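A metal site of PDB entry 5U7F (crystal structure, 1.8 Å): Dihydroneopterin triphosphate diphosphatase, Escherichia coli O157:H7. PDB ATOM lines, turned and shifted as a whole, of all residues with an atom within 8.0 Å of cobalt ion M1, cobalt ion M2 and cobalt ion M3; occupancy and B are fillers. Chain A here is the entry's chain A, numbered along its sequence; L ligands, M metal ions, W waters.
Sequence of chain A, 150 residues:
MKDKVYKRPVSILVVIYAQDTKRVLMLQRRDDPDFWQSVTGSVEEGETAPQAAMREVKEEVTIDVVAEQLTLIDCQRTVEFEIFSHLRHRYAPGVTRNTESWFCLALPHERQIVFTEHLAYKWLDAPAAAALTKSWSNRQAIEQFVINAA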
ATOM      1  N   LYS A   7     -14.112  30.888  21.126  1.00  0.00           N
ATOM      2  CA  LYS A   7     -12.725  31.048  21.520  1.00  0.00           C
ATOM      3  C   LYS A   7     -12.123  32.294  20.829  1.00  0.00           C
ATOM      4  O   LYS A   7     -12.502  32.621  19.702  1.00  0.00           O
ATOM      5  CB  LYS A   7     -11.923  29.806  21.141  1.00  0.00           C
ATOM      6  CG  LYS A   7     -12.039  28.619  22.074  1.00  0.00           C
ATOM      7  CD  LYS A   7     -10.882  27.639  21.830  1.00  0.00           C
ATOM      8  CE  LYS A   7     -10.674  26.720  23.034  1.00  0.00           C
ATOM      9  NZ  LYS A   7      -9.231  26.456  23.300  1.00  0.00           N
ATOM     10  N   ILE A  12      -1.828  32.003  23.938  1.00  0.00           N
ATOM     11  CA  ILE A  12      -0.512  31.821  24.500  1.00  0.00           C
ATOM     12  C   ILE A  12      -0.183  30.343  24.549  1.00  0.00           C
ATOM     13  O   ILE A  12      -1.066  29.484  24.542  1.00  0.00           O
ATOM     14  CB  ILE A  12      -0.380  32.479  25.900  1.00  0.00           C
ATOM     15  CG1 ILE A  12      -1.422  31.980  26.899  1.00  0.00           C
ATOM     16  CG2 ILE A  12      -0.493  33.998  25.781  1.00  0.00           C
ATOM     17  CD1 ILE A  12      -1.071  30.688  27.568  1.00  0.00           C
ATOM     18  N   LEU A  27       0.450  17.197  27.671  1.00  0.00           N
ATOM     19  CA  LEU A  27      -0.897  17.030  28.199  1.00  0.00           C
ATOM     20  C   LEU A  27      -1.803  16.588  27.067  1.00  0.00           C
ATOM     21  O   LEU A  27      -1.747  17.127  25.985  1.00  0.00           O
ATOM     22  CB  LEU A  27      -1.384  18.339  28.819  1.00  0.00           C
ATOM     23  CG  LEU A  27      -0.511  19.003  29.869  1.00  0.00           C
ATOM     24  CD1 LEU A  27      -0.924  20.429  30.106  1.00  0.00           C
ATOM     25  CD2 LEU A  27      -0.616  18.227  31.139  1.00  0.00           C
ATOM     26  N   ARG A  29      -5.210  16.258  25.107  1.00  0.00           N
ATOM     27  CA  ARG A  29      -6.432  17.048  25.027  1.00  0.00           C
ATOM     28  C   ARG A  29      -7.714  16.222  25.141  1.00  0.00           C
ATOM     29  O   ARG A  29      -7.727  15.027  24.823  1.00  0.00           O
ATOM     30  CB  ARG A  29      -6.502  17.841  23.720  1.00  0.00           C
ATOM     31  CG  ARG A  29      -5.523  18.972  23.668  1.00  0.00           C
ATOM     32  CD  ARG A  29      -5.823  19.882  22.464  1.00  0.00           C
ATOM     33  NE  ARG A  29      -7.127  20.520  22.598  1.00  0.00           N
ATOM     34  CZ  ARG A  29      -7.364  21.573  23.378  1.00  0.00           C
ATOM     35  NH1 ARG A  29      -6.393  22.101  24.123  1.00  0.00           N
ATOM     36  NH2 ARG A  29      -8.584  22.105  23.441  1.00  0.00           N
ATOM     37  N   GLN A  37       0.009  18.259  24.018  1.00  0.00           N
ATOM     38  CA  GLN A  37       0.498  19.646  23.932  1.00  0.00           C
ATOM     39  C   GLN A  37       1.031  20.149  25.246  1.00  0.00           C
ATOM     40  O   GLN A  37       0.724  19.588  26.305  1.00  0.00           O
ATOM     41  CB  GLN A  37      -0.644  20.562  23.497  1.00  0.00           C
ATOM     42  CG  GLN A  37      -1.851  20.450  24.380  1.00  0.00           C
ATOM     43  CD  GLN A  37      -2.830  21.596  24.259  1.00  0.00           C
ATOM     44  OE1 GLN A  37      -3.810  21.674  25.034  1.00  0.00           O
ATOM     45  NE2 GLN A  37      -2.630  22.454  23.268  1.00  0.00           N
ATOM     46  N   SER A  38       1.817  21.229  25.176  1.00  0.00           N
ATOM     47  CA  SER A  38       2.094  22.038  26.342  1.00  0.00           C
ATOM     48  C   SER A  38       0.833  22.867  26.689  1.00  0.00           C
ATOM     49  O   SER A  38      -0.242  22.685  26.073  1.00  0.00           O
ATOM     50  CB  SER A  38       3.320  22.956  26.085  1.00  0.00           C
ATOM     51  OG  SER A  38       4.357  22.231  25.415  1.00  0.00           O
ATOM     52  N   VAL A  39       0.903  23.721  27.712  1.00  0.00           N
ATOM     53  CA  VAL A  39      -0.238  24.548  28.085  1.00  0.00           C
ATOM     54  C   VAL A  39      -0.537  25.604  27.001  1.00  0.00           C
ATOM     55  O   VAL A  39       0.360  26.325  26.596  1.00  0.00           O
ATOM     56  CB  VAL A  39       0.006  25.212  29.433  1.00  0.00           C
ATOM     57  CG1 VAL A  39      -0.999  26.300  29.730  1.00  0.00           C
ATOM     58  CG2 VAL A  39      -0.051  24.158  30.539  1.00  0.00           C
ATOM     59  N   THR A  40      -1.772  25.660  26.497  1.00  0.00           N
ATOM     60  CA  THR A  40      -2.182  26.732  25.576  1.00  0.00           C
ATOM     61  C   THR A  40      -3.470  27.335  26.109  1.00  0.00           C
ATOM     62  O   THR A  40      -4.176  26.689  26.885  1.00  0.00           O
ATOM     63  CB  THR A  40      -2.405  26.260  24.108  1.00  0.00           C
ATOM     64  OG1 THR A  40      -3.533  25.394  24.035  1.00  0.00           O
ATOM     65  CG2 THR A  40      -1.177  25.573  23.557  1.00  0.00           C
ATOM     66  N   GLY A  41      -3.763  28.571  25.745  1.00  0.00           N
ATOM     67  CA  GLY A  41      -5.018  29.175  26.126  1.00  0.00           C
ATOM     68  C   GLY A  41      -5.239  30.502  25.445  1.00  0.00           C
ATOM     69  O   GLY A  41      -4.260  31.163  25.080  1.00  0.00           O
ATOM     70  N   SER A  42      -6.508  30.866  25.267  1.00  0.00           N
ATOM     71  CA  SER A  42      -6.879  32.168  24.713  1.00  0.00           C
ATOM     72  C   SER A  42      -6.571  33.322  25.664  1.00  0.00           C
ATOM     73  O   SER A  42      -6.718  33.202  26.876  1.00  0.00           O
ATOM     74  CB  SER A  42      -8.380  32.217  24.358  1.00  0.00           C
ATOM     75  OG  SER A  42      -8.689  31.354  23.276  1.00  0.00           O
ATOM     76  N   VAL A  43      -6.117  34.440  25.071  1.00  0.00           N
ATOM     77  CA  VAL A  43      -5.988  35.717  25.780  1.00  0.00           C
ATOM     78  C   VAL A  43      -7.338  36.401  25.801  1.00  0.00           C
ATOM     79  O   VAL A  43      -7.864  36.776  24.754  1.00  0.00           O
ATOM     80  CB  VAL A  43      -4.969  36.641  25.097  1.00  0.00           C
ATOM     81  CG1 VAL A  43      -4.788  37.934  25.894  1.00  0.00           C
ATOM     82  CG2 VAL A  43      -3.660  35.919  24.939  1.00  0.00           C
ATOM     83  N   GLU A  44      -7.887  36.584  26.998  1.00  0.00           N
ATOM     84  CA  GLU A  44      -9.218  37.189  27.115  1.00  0.00           C
ATOM     85  C   GLU A  44      -9.178  38.705  27.063  1.00  0.00           C
ATOM     86  O   GLU A  44      -8.152  39.324  27.301  1.00  0.00           O
ATOM     87  CB  GLU A  44      -9.890  36.747  28.416  1.00  0.00           C
ATOM     88  CG  GLU A  44     -10.035  35.236  28.547  1.00  0.00           C
ATOM     89  CD  GLU A  44     -10.900  34.607  27.444  1.00  0.00           C
ATOM     90  OE1 GLU A  44     -11.703  35.334  26.824  1.00  0.00           O
ATOM     91  OE2 GLU A  44     -10.781  33.386  27.189  1.00  0.00           O
ATOM     92  N   GLU A  47      -6.998  41.364  29.362  1.00  0.00           N
ATOM     93  CA  GLU A  47      -5.775  40.827  29.946  1.00  0.00           C
ATOM     94  C   GLU A  47      -4.628  40.787  28.928  1.00  0.00           C
ATOM     95  O   GLU A  47      -4.828  40.789  27.707  1.00  0.00           O
ATOM     96  CB  GLU A  47      -6.020  39.416  30.576  1.00  0.00           C
ATOM     97  CG  GLU A  47      -6.090  38.230  29.608  1.00  0.00           C
ATOM     98  CD  GLU A  47      -6.383  36.847  30.268  1.00  0.00           C
ATOM     99  OE1 GLU A  47      -6.084  36.636  31.480  1.00  0.00           O
ATOM    100  OE2 GLU A  47      -6.902  35.958  29.552  1.00  0.00           O
ATOM    101  N   ALA A  52      -2.370  36.020  30.808  1.00  0.00           N
ATOM    102  CA  ALA A  52      -3.134  34.876  30.354  1.00  0.00           C
ATOM    103  C   ALA A  52      -2.327  33.602  30.581  1.00  0.00           C
ATOM    104  O   ALA A  52      -2.851  32.582  31.003  1.00  0.00           O
ATOM    105  CB  ALA A  52      -3.509  35.042  28.874  1.00  0.00           C
ATOM    106  N   ARG A  55      -2.364  32.684  34.156  1.00  0.00           N
ATOM    107  CA  ARG A  55      -3.686  32.208  34.529  1.00  0.00           C
ATOM    108  C   ARG A  55      -3.914  30.791  34.057  1.00  0.00           C
ATOM    109  O   ARG A  55      -4.377  29.954  34.819  1.00  0.00           O
ATOM    110  CB  ARG A  55      -4.776  33.110  33.992  1.00  0.00           C
ATOM    111  CG  ARG A  55      -6.184  32.581  34.297  1.00  0.00           C
ATOM    112  CD  ARG A  55      -7.255  33.387  33.685  1.00  0.00           C
ATOM    113  NE  ARG A  55      -6.942  33.755  32.303  1.00  0.00           N
ATOM    114  CZ  ARG A  55      -7.092  32.951  31.262  1.00  0.00           C
ATOM    115  NH1 ARG A  55      -7.598  31.726  31.417  1.00  0.00           N
ATOM    116  NH2 ARG A  55      -6.767  33.387  30.059  1.00  0.00           N
ATOM    117  N   GLU A  56      -3.628  30.520  32.779  1.00  0.00           N
ATOM    118  CA  GLU A  56      -3.814  29.196  32.213  1.00  0.00           C
ATOM    119  C   GLU A  56      -2.924  28.151  32.895  1.00  0.00           C
ATOM    120  O   GLU A  56      -3.290  26.999  33.029  1.00  0.00           O
ATOM    121  CB  GLU A  56      -3.522  29.237  30.717  1.00  0.00           C
ATOM    122  CG  GLU A  56      -4.537  30.044  29.944  1.00  0.00           C
ATOM    123  CD  GLU A  56      -5.902  29.318  29.739  1.00  0.00           C
ATOM    124  OE1 GLU A  56      -5.933  28.104  29.921  1.00  0.00           O
ATOM    125  OE2 GLU A  56      -6.903  29.990  29.372  1.00  0.00           O
ATOM    126  N   VAL A  57      -1.733  28.560  33.339  1.00  0.00           N
ATOM    127  CA  VAL A  57      -0.853  27.608  33.996  1.00  0.00           C
ATOM    128  C   VAL A  57      -1.483  27.215  35.333  1.00  0.00           C
ATOM    129  O   VAL A  57      -1.472  26.033  35.709  1.00  0.00           O
ATOM    130  CB  VAL A  57       0.568  28.180  34.185  1.00  0.00           C
ATOM    131  CG1 VAL A  57       1.375  27.319  35.175  1.00  0.00           C
ATOM    132  CG2 VAL A  57       1.266  28.242  32.819  1.00  0.00           C
ATOM    133  N   GLU A  59      -4.833  27.385  36.075  1.00  0.00           N
ATOM    134  CA  GLU A  59      -6.053  26.615  35.704  1.00  0.00           C
ATOM    135  C   GLU A  59      -5.779  25.189  35.208  1.00  0.00           C
ATOM    136  O   GLU A  59      -6.476  24.253  35.603  1.00  0.00           O
ATOM    137  CB  GLU A  59      -6.853  27.360  34.614  1.00  0.00           C
ATOM    138  CG  GLU A  59      -7.521  28.674  35.048  1.00  0.00           C
ATOM    139  CD  GLU A  59      -8.286  29.398  33.913  1.00  0.00           C
ATOM    140  OE1 GLU A  59      -8.818  30.512  34.158  1.00  0.00           O
ATOM    141  OE2 GLU A  59      -8.363  28.852  32.787  1.00  0.00           O
ATOM    142  N   GLU A  60      -4.790  25.029  34.330  1.00  0.00           N
ATOM    143  CA  GLU A  60      -4.592  23.768  33.623  1.00  0.00           C
ATOM    144  C   GLU A  60      -3.696  22.753  34.297  1.00  0.00           C
ATOM    145  O   GLU A  60      -3.872  21.552  34.113  1.00  0.00           O
ATOM    146  CB  GLU A  60      -4.028  24.053  32.233  1.00  0.00           C
ATOM    147  CG  GLU A  60      -5.050  24.842  31.356  1.00  0.00           C
ATOM    148  CD  GLU A  60      -4.825  24.750  29.873  1.00  0.00           C
ATOM    149  OE1 GLU A  60      -3.836  24.142  29.463  1.00  0.00           O
ATOM    150  OE2 GLU A  60      -5.669  25.302  29.103  1.00  0.00           O
ATOM    151  N   THR A 116      -6.859  19.823  34.798  1.00  0.00           N
ATOM    152  CA  THR A 116      -8.292  20.102  34.736  1.00  0.00           C
ATOM    153  C   THR A 116      -8.874  20.029  33.308  1.00  0.00           C
ATOM    154  O   THR A 116      -9.978  19.519  33.091  1.00  0.00           O
ATOM    155  CB  THR A 116      -8.588  21.492  35.330  1.00  0.00           C
ATOM    156  OG1 THR A 116      -7.883  22.491  34.596  1.00  0.00           O
ATOM    157  CG2 THR A 116      -8.145  21.558  36.776  1.00  0.00           C
ATOM    158  N   GLU A 117      -8.122  20.519  32.332  1.00  0.00           N
ATOM    159  CA  GLU A 117      -8.580  20.636  30.961  1.00  0.00           C
ATOM    160  C   GLU A 117      -8.252  19.395  30.101  1.00  0.00           C
ATOM    161  O   GLU A 117      -8.719  19.270  28.965  1.00  0.00           O
ATOM    162  CB  GLU A 117      -7.941  21.916  30.337  1.00  0.00           C
ATOM    163  CG  GLU A 117      -8.411  22.307  28.943  1.00  0.00           C
ATOM    164  CD  GLU A 117      -7.804  23.651  28.466  1.00  0.00           C
ATOM    165  OE1 GLU A 117      -6.978  23.645  27.507  1.00  0.00           O
ATOM    166  OE2 GLU A 117      -8.157  24.710  29.056  1.00  0.00           O
ATOM    167  N   HIS A 118      -7.472  18.460  30.657  1.00  0.00           N
ATOM    168  CA  HIS A 118      -6.898  17.383  29.868  1.00  0.00           C
ATOM    169  C   HIS A 118      -7.271  15.981  30.393  1.00  0.00           C
ATOM    170  O   HIS A 118      -7.917  15.880  31.409  1.00  0.00           O
ATOM    171  CB  HIS A 118      -5.389  17.540  29.840  1.00  0.00           C
ATOM    172  CG  HIS A 118      -4.940  18.770  29.106  1.00  0.00           C
ATOM    173  ND1 HIS A 118      -4.911  20.018  29.696  1.00  0.00           N
ATOM    174  CD2 HIS A 118      -4.551  18.951  27.821  1.00  0.00           C
ATOM    175  CE1 HIS A 118      -4.490  20.910  28.821  1.00  0.00           C
ATOM    176  NE2 HIS A 118      -4.254  20.294  27.674  1.00  0.00           N
HETATM  177  S1  LIG L   1      -8.115  27.298  26.239  1.00  0.00           S
HETATM  178  O1  LIG L   1      -7.636  27.166  24.853  1.00  0.00           O
HETATM  179  O2  LIG L   1      -9.405  26.611  26.346  1.00  0.00           O
HETATM  180  O3  LIG L   1      -7.117  26.707  27.163  1.00  0.00           O
HETATM  181  O4  LIG L   1      -8.302  28.708  26.567  1.00  0.00           O
HETATM  182 CO    CO M   1      -5.623  25.241  27.028  1.00  0.00          CO
HETATM  183 CO    CO M   2      -7.267  26.630  29.361  1.00  0.00          CO
HETATM  184 CO    CO M   3      -8.805  29.583  28.507  1.00  0.00          CO
HETATM  185 CO    CO M   4     -10.602  27.206  28.058  1.00  0.00          CO
HETATM  186  O   HOH W   1     -10.929  29.306  27.716  1.00  0.00           O
HETATM  187  O   HOH W   2      -3.921  23.871  26.886  1.00  0.00           O
HETATM  188  O   HOH W   3      -8.811  27.774  29.398  1.00  0.00           O
HETATM  189  O   HOH W   4      -6.055  25.416  24.899  1.00  0.00           O
HETATM  190  O   HOH W   5      -9.696  30.121  30.406  1.00  0.00           O
HETATM  191  O   HOH W   6      -8.777  31.589  27.780  1.00  0.00           O
HETATM  192  O   HOH W   7      -7.792  26.438  31.431  1.00  0.00           O
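NE2 of Gln 37 lies within hydrogen-bond range of OG1 of Thr 40, 3.2 Å away. The side-chain carboxylate (OE2) of Glu 56 lies close to the guanidinium group (NH1) of Arg 55 (2.8 Å). The side-chain carboxylate (OE1) of Glu 117 lies close to the guanidinium group (NH1) of Arg 29. O of Ser 42 lies within hydrogen-bond range of NH2 of Arg 55 (3.2 Å). The guanidinium group of Arg 55 lies within salt-bridge range of the side-chain carboxylate of Glu 59, at 3.2 Å. OE2 of Glu 47 is in salt-bridge range of NH2 of Arg 55, at 2.6 Å.
Of the 22 residues printed, 4 come within 4 Å of cobalt ion M2.
Residues that only touch cobalt ion M3: Arg 55 (3.8 Å). Two residues have an atom within 4 Å of cobalt ion M3: Arg 55 and Glu 56. The nearest printed residue that does not touch cobalt ion M3 is Ser 42 (4.2 Å).
Cobalt ion M1 is bound by O of Thr 40 (2.1 Å), OE2 of Glu 60 (2.1 Å), O3 of the ligand (2.1 Å), OE1 of Glu 117 (2.1 Å), water W4 (2.2 Å) and water W2 (2.2 Å). Cobalt ion M1 has six donor atoms within binding distance.
Cobalt ion M2 is bound by water W3 (1.9 Å), OE1 of Glu 56 (2.1 Å), OE2 of Glu 60 (2.1 Å), OE2 of Glu 117 (2.1 Å), water W7 (2.1 Å) and O3 of the ligand (2.2 Å). Cobalt ion M2 has six donor atoms within binding distance.
Cobalt ion M3 is bound by water W3 (2.0 Å), OE2 of Glu 56 (2.1 Å), water W6 (2.1 Å), water W5 (2.2 Å), O4 of the ligand (2.2 Å) and water W1 (2.3 Å). Cobalt ion M3 has six donor atoms within binding distance.
Water W4 bridges the side-chain hydroxyl of Thr 40 (2.7 Å) and the guanidinium group of Arg 29 (3.4 Å). Water W2 lies within hydrogen-bond range of the side-chain carboxylate of Glu 60 (2.6 Å), the backbone NH of Thr 40 (2.8 Å) and the side-chain amide oxygen of Gln 37 (2.9 Å). Water W5 bridges NH1 of Arg 55 (2.8 Å) and OE2 of Glu 59 (3.0 Å). Water W6 lies within hydrogen-bond range of OE2 of Glu 44 and O of Ser 42.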
